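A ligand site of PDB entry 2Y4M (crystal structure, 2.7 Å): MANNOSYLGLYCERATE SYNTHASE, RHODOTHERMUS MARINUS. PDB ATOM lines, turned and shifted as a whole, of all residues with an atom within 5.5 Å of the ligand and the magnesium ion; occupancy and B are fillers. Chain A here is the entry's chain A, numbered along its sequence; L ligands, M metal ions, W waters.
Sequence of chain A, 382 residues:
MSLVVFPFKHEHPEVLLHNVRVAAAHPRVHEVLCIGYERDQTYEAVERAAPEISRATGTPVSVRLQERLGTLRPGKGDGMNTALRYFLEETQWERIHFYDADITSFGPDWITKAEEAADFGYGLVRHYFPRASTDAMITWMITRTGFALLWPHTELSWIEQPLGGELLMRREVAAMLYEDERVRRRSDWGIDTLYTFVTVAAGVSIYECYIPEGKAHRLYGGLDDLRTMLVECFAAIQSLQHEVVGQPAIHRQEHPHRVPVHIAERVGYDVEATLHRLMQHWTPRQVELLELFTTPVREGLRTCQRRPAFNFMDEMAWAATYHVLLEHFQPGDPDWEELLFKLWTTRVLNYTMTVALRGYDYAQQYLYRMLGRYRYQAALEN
The backbone carbonyl oxygen of Gly 75 sits close to an oxygen (O1) of the ligand.
Residues that only touch the ligand: Tyr 37, Met 229, Gly 164, Trp 189, Lys 215, Gly 36 and Gly 79.
Hydrophobic or aromatic side chains that line the ligand: Pro 7, Tyr 37, Ala 101, Leu 163, Trp 189, His 217 and Met 229.
Of the 31 residues printed, 23 come within 4 Å of the ligand.
NE2 of Gln 66 is in hydrogen-bond range of O of Gly 75, at 3.1 Å.
O of Gly 36 is in hydrogen-bond range of N of Gln 66, 2.9 Å away.
The side-chain carboxylate (OE2) of Glu 11 lies within salt-bridge range of the guanidinium group (NH1) of Arg 218, at 3.1 Å.
The side-chain carboxylate of Asp 192 is in salt-bridge range of the side-chain amino group of Lys 76 (2.7 Å).
The backbone NH (N) of Asp 100 lies within hydrogen-bond range of the side-chain carboxylate (OE2) of Glu 166, at 3.0 Å.
O of Ile 35 lies within hydrogen-bond range of N of Phe 8.
The backbone carbonyl oxygen of Met 229 sits close to the side-chain sulfur of Cys 233 (3.3 Å).
NZ of Lys 215 is in salt-bridge range of OE1 of Glu 166, at 2.9 Å.
OE1 of Gln 66 sits at hydrogen-bond distance from N2 of the ligand (2.4 Å).
OE2 of Glu 11 sits at hydrogen-bond distance from O2 of the ligand.
An oxygen (O16) of the ligand sits at hydrogen-bond distance from the side-chain carboxylate (OD2) of Asp 192 (2.6 Å).
The side-chain carboxylate of Asp 100 lies within hydrogen-bond range of an oxygen (O15) of the ligand (2.6 Å).
The backbone carbonyl oxygen of Ile 35 is in hydrogen-bond range of a nitrogen (N1) of the ligand (2.7 Å).
O of Pro 7 sits at hydrogen-bond distance from O3 of the ligand, at 2.7 Å.
O2 of the ligand lies within hydrogen-bond range of N of Lys 9 (2.9 Å).
The backbone NH (N) of Ala 101 sits at hydrogen-bond distance from an oxygen (O3) of the ligand.
The backbone NH (N) of Lys 76 sits at hydrogen-bond distance from an oxygen (O1) of the ligand (3.1 Å).
An oxygen (O16) of the ligand sits at hydrogen-bond distance from the side-chain amino group (NZ) of Lys 76, 2.9 Å away.
The backbone carbonyl oxygen (O) of Leu 163 sits at hydrogen-bond distance from an oxygen (O14) of the ligand, at 3.1 Å.
The backbone NH (N) of Phe 8 lies close to a nitrogen (N3) of the ligand (3.5 Å).
A nitrogen (N1) of the ligand lies within hydrogen-bond range of the backbone carbonyl oxygen (O) of Phe 8 (3.4 Å).
An oxygen (O14) of the ligand is in hydrogen-bond range of the backbone NH of Gly 165.
The guanidinium group (NH2) of Arg 218 lies within salt-bridge range of an oxygen (O7) of the ligand, 3.5 Å away.
The magnesium ion is bound by an oxygen (O10) of the ligand, the side-chain carboxylate of Asp 102, water W1, an oxygen (O6) of the ligand, a ring nitrogen (ND1) of His 217 and water W3.
The magnesium ion has six donor atoms within binding distance.
Water W3 bridges OD1 of Asp 102 (2.4 Å) and OD2 of Asp 100 (2.8 Å).
Of the 31 residues printed, 2 come within 4 Å of the magnesium ion.
The nearest printed residue that does not touch the magnesium ion is Arg 218 (4.1 Å).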
ATOM      1  N   PRO A   7      22.874  16.679  13.338  1.00  0.00           N
ATOM      2  CA  PRO A   7      22.377  18.024  13.546  1.00  0.00           C
ATOM      3  C   PRO A   7      22.362  18.378  15.010  1.00  0.00           C
ATOM      4  O   PRO A   7      21.832  17.621  15.829  1.00  0.00           O
ATOM      5  CB  PRO A   7      20.947  17.946  13.035  1.00  0.00           C
ATOM      6  CG  PRO A   7      20.735  16.564  12.588  1.00  0.00           C
ATOM      7  CD  PRO A   7      21.789  15.722  13.120  1.00  0.00           C
ATOM      8  N   PHE A   8      22.890  19.532  15.351  1.00  0.00           N
ATOM      9  CA  PHE A   8      22.927  19.923  16.757  1.00  0.00           C
ATOM     10  C   PHE A   8      22.532  21.365  17.019  1.00  0.00           C
ATOM     11  O   PHE A   8      22.828  22.251  16.214  1.00  0.00           O
ATOM     12  CB  PHE A   8      24.311  19.645  17.352  1.00  0.00           C
ATOM     13  CG  PHE A   8      25.375  20.560  16.855  1.00  0.00           C
ATOM     14  CD1 PHE A   8      26.032  20.294  15.649  1.00  0.00           C
ATOM     15  CD2 PHE A   8      25.765  21.679  17.606  1.00  0.00           C
ATOM     16  CE1 PHE A   8      27.033  21.118  15.192  1.00  0.00           C
ATOM     17  CE2 PHE A   8      26.765  22.504  17.159  1.00  0.00           C
ATOM     18  CZ  PHE A   8      27.403  22.227  15.942  1.00  0.00           C
ATOM     19  N   LYS A   9      21.870  21.573  18.148  1.00  0.00           N
ATOM     20  CA  LYS A   9      21.516  22.895  18.596  1.00  0.00           C
ATOM     21  C   LYS A   9      22.309  23.113  19.861  1.00  0.00           C
ATOM     22  O   LYS A   9      23.464  23.567  19.805  1.00  0.00           O
ATOM     23  CB  LYS A   9      20.007  23.037  18.836  1.00  0.00           C
ATOM     24  CG  LYS A   9      19.546  24.467  18.990  1.00  0.00           C
ATOM     25  CD  LYS A   9      18.070  24.608  19.254  1.00  0.00           C
ATOM     26  CE  LYS A   9      17.727  26.075  19.267  1.00  0.00           C
ATOM     27  NZ  LYS A   9      16.347  26.486  18.934  1.00  0.00           N
ATOM     28  N   HIS A  10      21.719  22.751  20.994  1.00  0.00           N
ATOM     29  CA  HIS A  10      22.352  22.966  22.291  1.00  0.00           C
ATOM     30  C   HIS A  10      22.670  21.652  23.020  1.00  0.00           C
ATOM     31  O   HIS A  10      21.906  21.197  23.878  1.00  0.00           O
ATOM     32  CB  HIS A  10      21.462  23.864  23.156  1.00  0.00           C
ATOM     33  CG  HIS A  10      21.322  25.255  22.614  1.00  0.00           C
ATOM     34  ND1 HIS A  10      20.137  25.967  22.693  1.00  0.00           N
ATOM     35  CD2 HIS A  10      22.214  26.063  21.984  1.00  0.00           C
ATOM     36  CE1 HIS A  10      20.307  27.161  22.141  1.00  0.00           C
ATOM     37  NE2 HIS A  10      21.556  27.231  21.692  1.00  0.00           N
ATOM     38  N   GLU A  11      23.797  21.035  22.674  1.00  0.00           N
ATOM     39  CA  GLU A  11      24.104  19.692  23.192  1.00  0.00           C
ATOM     40  C   GLU A  11      25.345  19.736  24.047  1.00  0.00           C
ATOM     41  O   GLU A  11      26.138  20.666  23.931  1.00  0.00           O
ATOM     42  CB  GLU A  11      24.289  18.730  22.019  1.00  0.00           C
ATOM     43  CG  GLU A  11      23.145  18.739  20.988  1.00  0.00           C
ATOM     44  CD  GLU A  11      21.854  18.172  21.542  1.00  0.00           C
ATOM     45  OE1 GLU A  11      21.908  17.484  22.584  1.00  0.00           O
ATOM     46  OE2 GLU A  11      20.766  18.413  20.974  1.00  0.00           O
ATOM     47  N   ILE A  35      26.102  19.672  11.991  1.00  0.00           N
ATOM     48  CA  ILE A  35      25.378  20.792  11.434  1.00  0.00           C
ATOM     49  C   ILE A  35      24.648  21.554  12.530  1.00  0.00           C
ATOM     50  O   ILE A  35      23.615  21.118  13.053  1.00  0.00           O
ATOM     51  CB  ILE A  35      24.501  20.361  10.227  1.00  0.00           C
ATOM     52  CG1 ILE A  35      23.947  21.591   9.539  1.00  0.00           C
ATOM     53  CG2 ILE A  35      23.394  19.416  10.621  1.00  0.00           C
ATOM     54  CD1 ILE A  35      25.017  22.302   8.776  1.00  0.00           C
ATOM     55  N   GLY A  36      25.226  22.695  12.888  1.00  0.00           N
ATOM     56  CA  GLY A  36      24.857  23.434  14.068  1.00  0.00           C
ATOM     57  C   GLY A  36      23.832  24.492  13.794  1.00  0.00           C
ATOM     58  O   GLY A  36      23.766  25.051  12.701  1.00  0.00           O
ATOM     59  N   TYR A  37      23.018  24.741  14.812  1.00  0.00           N
ATOM     60  CA  TYR A  37      22.112  25.870  14.818  1.00  0.00           C
ATOM     61  C   TYR A  37      22.893  27.173  14.721  1.00  0.00           C
ATOM     62  O   TYR A  37      22.654  27.964  13.812  1.00  0.00           O
ATOM     63  CB  TYR A  37      21.270  25.862  16.106  1.00  0.00           C
ATOM     64  CG  TYR A  37      20.300  27.026  16.264  1.00  0.00           C
ATOM     65  CD1 TYR A  37      19.060  27.018  15.638  1.00  0.00           C
ATOM     66  CD2 TYR A  37      20.615  28.125  17.069  1.00  0.00           C
ATOM     67  CE1 TYR A  37      18.152  28.060  15.782  1.00  0.00           C
ATOM     68  CE2 TYR A  37      19.710  29.190  17.232  1.00  0.00           C
ATOM     69  CZ  TYR A  37      18.476  29.153  16.579  1.00  0.00           C
ATOM     70  OH  TYR A  37      17.562  30.186  16.724  1.00  0.00           O
ATOM     71  N   GLN A  66      23.956  25.891   9.928  1.00  0.00           N
ATOM     72  CA  GLN A  66      22.767  25.758   9.106  1.00  0.00           C
ATOM     73  C   GLN A  66      22.424  27.078   8.404  1.00  0.00           C
ATOM     74  O   GLN A  66      22.484  28.147   9.011  1.00  0.00           O
ATOM     75  CB  GLN A  66      21.576  25.264   9.918  1.00  0.00           C
ATOM     76  CG  GLN A  66      20.998  26.263  10.882  1.00  0.00           C
ATOM     77  CD  GLN A  66      19.896  25.677  11.722  1.00  0.00           C
ATOM     78  OE1 GLN A  66      20.075  24.620  12.333  1.00  0.00           O
ATOM     79  NE2 GLN A  66      18.749  26.348  11.769  1.00  0.00           N
ATOM     80  N   ARG A  73       9.713  28.691  10.937  1.00  0.00           N
ATOM     81  CA  ARG A  73      10.705  28.935  11.980  1.00  0.00           C
ATOM     82  C   ARG A  73      12.111  28.396  11.609  1.00  0.00           C
ATOM     83  O   ARG A  73      12.260  27.267  11.143  1.00  0.00           O
ATOM     84  CB  ARG A  73      10.269  28.342  13.331  1.00  0.00           C
ATOM     85  CG  ARG A  73      11.064  28.873  14.571  1.00  0.00           C
ATOM     86  CD  ARG A  73      10.651  28.211  15.921  1.00  0.00           C
ATOM     87  NE  ARG A  73      10.502  26.768  15.718  1.00  0.00           N
ATOM     88  CZ  ARG A  73      11.488  25.866  15.803  1.00  0.00           C
ATOM     89  NH1 ARG A  73      12.706  26.232  16.165  1.00  0.00           N
ATOM     90  NH2 ARG A  73      11.245  24.583  15.526  1.00  0.00           N
ATOM     91  N   PRO A  74      13.161  29.217  11.794  1.00  0.00           N
ATOM     92  CA  PRO A  74      14.474  28.597  11.531  1.00  0.00           C
ATOM     93  C   PRO A  74      14.826  27.543  12.616  1.00  0.00           C
ATOM     94  O   PRO A  74      15.167  27.905  13.756  1.00  0.00           O
ATOM     95  CB  PRO A  74      15.466  29.802  11.547  1.00  0.00           C
ATOM     96  CG  PRO A  74      14.738  30.891  12.314  1.00  0.00           C
ATOM     97  CD  PRO A  74      13.253  30.652  12.143  1.00  0.00           C
ATOM     98  N   GLY A  75      14.697  26.261  12.271  1.00  0.00           N
ATOM     99  CA  GLY A  75      14.938  25.142  13.197  1.00  0.00           C
ATOM    100  C   GLY A  75      15.687  23.999  12.578  1.00  0.00           C
ATOM    101  O   GLY A  75      16.546  24.205  11.690  1.00  0.00           O
ATOM    102  N   LYS A  76      15.353  22.780  13.022  1.00  0.00           N
ATOM    103  CA  LYS A  76      16.065  21.550  12.597  1.00  0.00           C
ATOM    104  C   LYS A  76      15.972  21.278  11.084  1.00  0.00           C
ATOM    105  O   LYS A  76      16.960  20.806  10.498  1.00  0.00           O
ATOM    106  CB  LYS A  76      15.597  20.305  13.402  1.00  0.00           C
ATOM    107  CG  LYS A  76      16.397  18.969  13.097  1.00  0.00           C
ATOM    108  CD  LYS A  76      15.598  17.728  13.490  1.00  0.00           C
ATOM    109  CE  LYS A  76      16.360  16.395  13.272  1.00  0.00           C
ATOM    110  NZ  LYS A  76      15.390  15.327  12.793  1.00  0.00           N
ATOM    111  N   GLY A  79      18.743  22.800   9.289  1.00  0.00           N
ATOM    112  CA  GLY A  79      19.950  22.005   9.522  1.00  0.00           C
ATOM    113  C   GLY A  79      20.025  20.823   8.596  1.00  0.00           C
ATOM    114  O   GLY A  79      21.050  20.600   7.934  1.00  0.00           O
ATOM    115  N   TYR A  99      21.854  11.117  12.299  1.00  0.00           N
ATOM    116  CA  TYR A  99      21.608  10.629  13.674  1.00  0.00           C
ATOM    117  C   TYR A  99      21.504  11.808  14.607  1.00  0.00           C
ATOM    118  O   TYR A  99      22.322  12.732  14.534  1.00  0.00           O
ATOM    119  CB  TYR A  99      22.709   9.676  14.180  1.00  0.00           C
ATOM    120  CG  TYR A  99      22.832   8.456  13.324  1.00  0.00           C
ATOM    121  CD1 TYR A  99      21.941   7.399  13.449  1.00  0.00           C
ATOM    122  CD2 TYR A  99      23.827   8.371  12.354  1.00  0.00           C
ATOM    123  CE1 TYR A  99      22.026   6.271  12.631  1.00  0.00           C
ATOM    124  CE2 TYR A  99      23.935   7.239  11.529  1.00  0.00           C
ATOM    125  CZ  TYR A  99      23.019   6.200  11.660  1.00  0.00           C
ATOM    126  OH  TYR A  99      23.102   5.100  10.830  1.00  0.00           O
ATOM    127  N   ASP A 100      20.514  11.828  15.481  1.00  0.00           N
ATOM    128  CA  ASP A 100      20.474  12.883  16.451  1.00  0.00           C
ATOM    129  C   ASP A 100      21.770  12.972  17.259  1.00  0.00           C
ATOM    130  O   ASP A 100      22.385  11.975  17.602  1.00  0.00           O
ATOM    131  CB  ASP A 100      19.270  12.775  17.342  1.00  0.00           C
ATOM    132  CG  ASP A 100      18.009  13.173  16.640  1.00  0.00           C
ATOM    133  OD1 ASP A 100      18.096  13.655  15.490  1.00  0.00           O
ATOM    134  OD2 ASP A 100      16.928  12.974  17.229  1.00  0.00           O
ATOM    135  N   ALA A 101      22.163  14.204  17.547  1.00  0.00           N
ATOM    136  CA  ALA A 101      23.331  14.492  18.355  1.00  0.00           C
ATOM    137  C   ALA A 101      23.199  14.094  19.836  1.00  0.00           C
ATOM    138  O   ALA A 101      24.177  13.698  20.424  1.00  0.00           O
ATOM    139  CB  ALA A 101      23.685  15.970  18.205  1.00  0.00           C
ATOM    140  N   ASP A 102      22.016  14.211  20.428  1.00  0.00           N
ATOM    141  CA  ASP A 102      21.801  13.926  21.851  1.00  0.00           C
ATOM    142  C   ASP A 102      21.921  12.451  22.216  1.00  0.00           C
ATOM    143  O   ASP A 102      21.966  12.120  23.409  1.00  0.00           O
ATOM    144  CB  ASP A 102      20.443  14.479  22.367  1.00  0.00           C
ATOM    145  CG  ASP A 102      19.261  14.076  21.497  1.00  0.00           C
ATOM    146  OD1 ASP A 102      19.438  13.546  20.368  1.00  0.00           O
ATOM    147  OD2 ASP A 102      18.117  14.278  21.945  1.00  0.00           O
ATOM    148  N   LEU A 163       8.594  10.333  12.621  1.00  0.00           N
ATOM    149  CA  LEU A 163       9.280  11.529  13.108  1.00  0.00           C
ATOM    150  C   LEU A 163      10.723  11.259  13.477  1.00  0.00           C
ATOM    151  O   LEU A 163      11.397  12.163  13.995  1.00  0.00           O
ATOM    152  CB  LEU A 163       8.610  12.057  14.361  1.00  0.00           C
ATOM    153  CG  LEU A 163       7.149  12.478  14.251  1.00  0.00           C
ATOM    154  CD1 LEU A 163       6.723  13.285  15.469  1.00  0.00           C
ATOM    155  CD2 LEU A 163       6.922  13.300  12.966  1.00  0.00           C
ATOM    156  N   GLY A 164      11.218  10.054  13.237  1.00  0.00           N
ATOM    157  CA  GLY A 164      12.531   9.706  13.789  1.00  0.00           C
ATOM    158  C   GLY A 164      13.626  10.298  12.948  1.00  0.00           C
ATOM    159  O   GLY A 164      13.536  10.260  11.709  1.00  0.00           O
ATOM    160  N   GLY A 165      14.638  10.843  13.595  1.00  0.00           N
ATOM    161  CA  GLY A 165      15.763  11.461  12.907  1.00  0.00           C
ATOM    162  C   GLY A 165      16.936  10.546  12.600  1.00  0.00           C
ATOM    163  O   GLY A 165      18.028  11.024  12.212  1.00  0.00           O
ATOM    164  N   GLU A 166      16.759   9.235  12.757  1.00  0.00           N
ATOM    165  CA  GLU A 166      17.870   8.341  12.462  1.00  0.00           C
ATOM    166  C   GLU A 166      17.545   7.641  11.209  1.00  0.00           C
ATOM    167  O   GLU A 166      16.559   6.934  11.153  1.00  0.00           O
ATOM    168  CB  GLU A 166      18.103   7.340  13.580  1.00  0.00           C
ATOM    169  CG  GLU A 166      18.629   7.963  14.872  1.00  0.00           C
ATOM    170  CD  GLU A 166      17.639   8.938  15.487  1.00  0.00           C
ATOM    171  OE1 GLU A 166      16.432   8.625  15.576  1.00  0.00           O
ATOM    172  OE2 GLU A 166      18.078  10.047  15.841  1.00  0.00           O
ATOM    173  N   TRP A 189      10.354  21.972  12.969  1.00  0.00           N
ATOM    174  CA  TRP A 189      10.281  20.580  13.417  1.00  0.00           C
ATOM    175  C   TRP A 189       9.551  19.683  12.386  1.00  0.00           C
ATOM    176  O   TRP A 189       9.526  18.470  12.543  1.00  0.00           O
ATOM    177  CB  TRP A 189       9.565  20.450  14.759  1.00  0.00           C
ATOM    178  CG  TRP A 189      10.361  20.843  15.970  1.00  0.00           C
ATOM    179  CD1 TRP A 189      10.063  21.856  16.853  1.00  0.00           C
ATOM    180  CD2 TRP A 189      11.547  20.227  16.449  1.00  0.00           C
ATOM    181  NE1 TRP A 189      11.027  21.933  17.836  1.00  0.00           N
ATOM    182  CE2 TRP A 189      11.944  20.935  17.618  1.00  0.00           C
ATOM    183  CE3 TRP A 189      12.324  19.160  15.998  1.00  0.00           C
ATOM    184  CZ2 TRP A 189      13.092  20.610  18.341  1.00  0.00           C
ATOM    185  CZ3 TRP A 189      13.467  18.814  16.733  1.00  0.00           C
ATOM    186  CH2 TRP A 189      13.843  19.539  17.878  1.00  0.00           C
ATOM    187  N   ILE A 191      10.346  19.033   9.460  1.00  0.00           N
ATOM    188  CA  ILE A 191      11.206  18.448   8.465  1.00  0.00           C
ATOM    189  C   ILE A 191      11.022  16.943   8.334  1.00  0.00           C
ATOM    190  O   ILE A 191      10.831  16.454   7.231  1.00  0.00           O
ATOM    191  CB  ILE A 191      12.675  18.825   8.674  1.00  0.00           C
ATOM    192  CG1 ILE A 191      13.546  18.333   7.511  1.00  0.00           C
ATOM    193  CG2 ILE A 191      13.190  18.287   9.978  1.00  0.00           C
ATOM    194  CD1 ILE A 191      13.057  18.775   6.147  1.00  0.00           C
ATOM    195  N   ASP A 192      11.035  16.222   9.464  1.00  0.00           N
ATOM    196  CA  ASP A 192      11.001  14.729   9.470  1.00  0.00           C
ATOM    197  C   ASP A 192       9.728  14.180   8.844  1.00  0.00           C
ATOM    198  O   ASP A 192       9.804  13.273   8.028  1.00  0.00           O
ATOM    199  CB  ASP A 192      11.159  14.197  10.885  1.00  0.00           C
ATOM    200  CG  ASP A 192      12.405  14.753  11.548  1.00  0.00           C
ATOM    201  OD1 ASP A 192      13.519  14.311  11.166  1.00  0.00           O
ATOM    202  OD2 ASP A 192      12.276  15.650  12.410  1.00  0.00           O
ATOM    203  N   LYS A 215      16.902   3.968  22.167  1.00  0.00           N
ATOM    204  CA  LYS A 215      17.499   5.275  21.837  1.00  0.00           C
ATOM    205  C   LYS A 215      17.545   6.125  23.086  1.00  0.00           C
ATOM    206  O   LYS A 215      16.524   6.685  23.520  1.00  0.00           O
ATOM    207  CB  LYS A 215      16.739   6.023  20.740  1.00  0.00           C
ATOM    208  CG  LYS A 215      17.334   7.394  20.334  1.00  0.00           C
ATOM    209  CD  LYS A 215      16.352   8.222  19.477  1.00  0.00           C
ATOM    210  CE  LYS A 215      16.907   9.587  19.057  1.00  0.00           C
ATOM    211  NZ  LYS A 215      16.047  10.234  18.017  1.00  0.00           N
ATOM    212  N   HIS A 217      18.569   9.394  24.776  1.00  0.00           N
ATOM    213  CA  HIS A 217      18.828  10.831  24.548  1.00  0.00           C
ATOM    214  C   HIS A 217      18.239  11.687  25.683  1.00  0.00           C
ATOM    215  O   HIS A 217      17.649  11.113  26.622  1.00  0.00           O
ATOM    216  CB  HIS A 217      18.260  11.272  23.195  1.00  0.00           C
ATOM    217  CG  HIS A 217      16.790  11.021  23.037  1.00  0.00           C
ATOM    218  ND1 HIS A 217      15.903  12.000  22.644  1.00  0.00           N
ATOM    219  CD2 HIS A 217      16.057   9.894  23.186  1.00  0.00           C
ATOM    220  CE1 HIS A 217      14.686  11.481  22.556  1.00  0.00           C
ATOM    221  NE2 HIS A 217      14.751  10.211  22.889  1.00  0.00           N
ATOM    222  N   ARG A 218      18.375  13.029  25.600  1.00  0.00           N
ATOM    223  CA  ARG A 218      17.838  14.022  26.599  1.00  0.00           C
ATOM    224  C   ARG A 218      16.297  13.999  26.889  1.00  0.00           C
ATOM    225  O   ARG A 218      15.495  13.911  25.946  1.00  0.00           O
ATOM    226  CB  ARG A 218      18.207  15.453  26.152  1.00  0.00           C
ATOM    227  CG  ARG A 218      19.484  16.086  26.762  1.00  0.00           C
ATOM    228  CD  ARG A 218      19.868  17.419  26.021  1.00  0.00           C
ATOM    229  NE  ARG A 218      18.698  18.224  25.620  1.00  0.00           N
ATOM    230  CZ  ARG A 218      18.267  18.384  24.366  1.00  0.00           C
ATOM    231  NH1 ARG A 218      18.883  17.808  23.352  1.00  0.00           N
ATOM    232  NH2 ARG A 218      17.189  19.130  24.131  1.00  0.00           N
ATOM    233  N   LEU A 226       7.082  20.582  24.805  1.00  0.00           N
ATOM    234  CA  LEU A 226       6.775  19.919  23.531  1.00  0.00           C
ATOM    235  C   LEU A 226       5.822  20.687  22.612  1.00  0.00           C
ATOM    236  O   LEU A 226       5.458  20.242  21.526  1.00  0.00           O
ATOM    237  CB  LEU A 226       6.173  18.528  23.817  1.00  0.00           C
ATOM    238  CG  LEU A 226       7.120  17.353  24.172  1.00  0.00           C
ATOM    239  CD1 LEU A 226       6.338  16.038  24.219  1.00  0.00           C
ATOM    240  CD2 LEU A 226       8.427  17.181  23.286  1.00  0.00           C
ATOM    241  N   MET A 229       6.880  21.751  18.971  1.00  0.00           N
ATOM    242  CA  MET A 229       6.970  20.557  18.200  1.00  0.00           C
ATOM    243  C   MET A 229       5.597  20.007  17.855  1.00  0.00           C
ATOM    244  O   MET A 229       5.347  19.601  16.728  1.00  0.00           O
ATOM    245  CB  MET A 229       7.789  19.539  18.952  1.00  0.00           C
ATOM    246  CG  MET A 229       8.266  18.428  18.067  1.00  0.00           C
ATOM    247  SD  MET A 229       9.064  17.086  18.974  1.00  0.00           S
ATOM    248  CE  MET A 229      10.638  17.821  19.488  1.00  0.00           C
ATOM    249  N   CYS A 233       4.591  19.841  13.986  1.00  0.00           N
ATOM    250  CA  CYS A 233       4.277  18.550  13.429  1.00  0.00           C
ATOM    251  C   CYS A 233       2.823  18.503  12.974  1.00  0.00           C
ATOM    252  O   CYS A 233       2.511  17.880  11.979  1.00  0.00           O
ATOM    253  CB  CYS A 233       4.574  17.439  14.432  1.00  0.00           C
ATOM    254  SG  CYS A 233       6.319  17.216  14.731  1.00  0.00           S
HETATM  255  N1  LIG L   1      21.105  21.983  13.311  1.00  0.00           N
HETATM  256  C1  LIG L   1      20.012  22.081  14.107  1.00  0.00           C
HETATM  257  N2  LIG L   1      19.165  23.228  14.069  1.00  0.00           N
HETATM  258  N3  LIG L   1      19.802  21.067  14.943  1.00  0.00           N
HETATM  259  C2  LIG L   1      18.757  21.053  15.774  1.00  0.00           C
HETATM  260  C3  LIG L   1      17.875  22.101  15.800  1.00  0.00           C
HETATM  261  C4  LIG L   1      18.080  23.194  14.967  1.00  0.00           C
HETATM  262  O1  LIG L   1      17.271  24.148  15.039  1.00  0.00           O
HETATM  263  N4  LIG L   1      16.922  21.815  16.724  1.00  0.00           N
HETATM  264  C5  LIG L   1      17.226  20.600  17.241  1.00  0.00           C
HETATM  265  N5  LIG L   1      18.347  20.154  16.658  1.00  0.00           N
HETATM  266  C6  LIG L   1      19.011  18.856  16.860  1.00  0.00           C
HETATM  267  C7  LIG L   1      19.182  18.566  18.306  1.00  0.00           C
HETATM  268  O2  LIG L   1      20.426  19.150  18.674  1.00  0.00           O
HETATM  269  C8  LIG L   1      19.118  17.044  18.291  1.00  0.00           C
HETATM  270  O3  LIG L   1      20.330  16.439  17.802  1.00  0.00           O
HETATM  271  C9  LIG L   1      18.097  16.709  17.232  1.00  0.00           C
HETATM  272  O4  LIG L   1      18.093  17.861  16.401  1.00  0.00           O
HETATM  273  C10 LIG L   1      16.721  16.420  17.815  1.00  0.00           C
HETATM  274  O5  LIG L   1      16.518  17.373  18.835  1.00  0.00           O
HETATM  275  P1  LIG L   1      15.924  16.974  20.263  1.00  0.00           P
HETATM  276  O6  LIG L   1      16.733  15.803  20.764  1.00  0.00           O
HETATM  277  O7  LIG L   1      15.813  18.247  21.066  1.00  0.00           O
HETATM  278  O8  LIG L   1      14.461  16.443  19.856  1.00  0.00           O
HETATM  279  P2  LIG L   1      13.709  15.079  20.244  1.00  0.00           P
HETATM  280  O9  LIG L   1      12.652  15.487  21.231  1.00  0.00           O
HETATM  281  O10 LIG L   1      14.640  13.941  20.554  1.00  0.00           O
HETATM  282  O11 LIG L   1      12.969  14.720  18.856  1.00  0.00           O
HETATM  283  C11 LIG L   1      12.585  13.470  18.226  1.00  0.00           C
HETATM  284  O12 LIG L   1      11.468  13.710  17.322  1.00  0.00           O
HETATM  285  C12 LIG L   1      11.623  14.841  16.430  1.00  0.00           C
HETATM  286  C13 LIG L   1      10.328  15.064  15.667  1.00  0.00           C
HETATM  287  O13 LIG L   1      10.281  15.422  14.462  1.00  0.00           O
HETATM  288  C14 LIG L   1      13.699  13.030  17.279  1.00  0.00           C
HETATM  289  O14 LIG L   1      13.289  11.903  16.465  1.00  0.00           O
HETATM  290  C15 LIG L   1      14.072  14.210  16.378  1.00  0.00           C
HETATM  291  O15 LIG L   1      15.210  13.927  15.541  1.00  0.00           O
HETATM  292  C16 LIG L   1      12.866  14.630  15.529  1.00  0.00           C
HETATM  293  O16 LIG L   1      13.254  15.797  14.772  1.00  0.00           O
HETATM  294 MG    MG M   1      16.025  14.173  21.916  1.00  0.00          MG
HETATM  295  O   HOH W   1      16.562  15.174  23.694  1.00  0.00           O
HETATM  296  O   HOH W   2      16.580  20.695  20.522  1.00  0.00           O
HETATM  297  O   HOH W   3      17.053  13.164  20.005  1.00  0.00           O
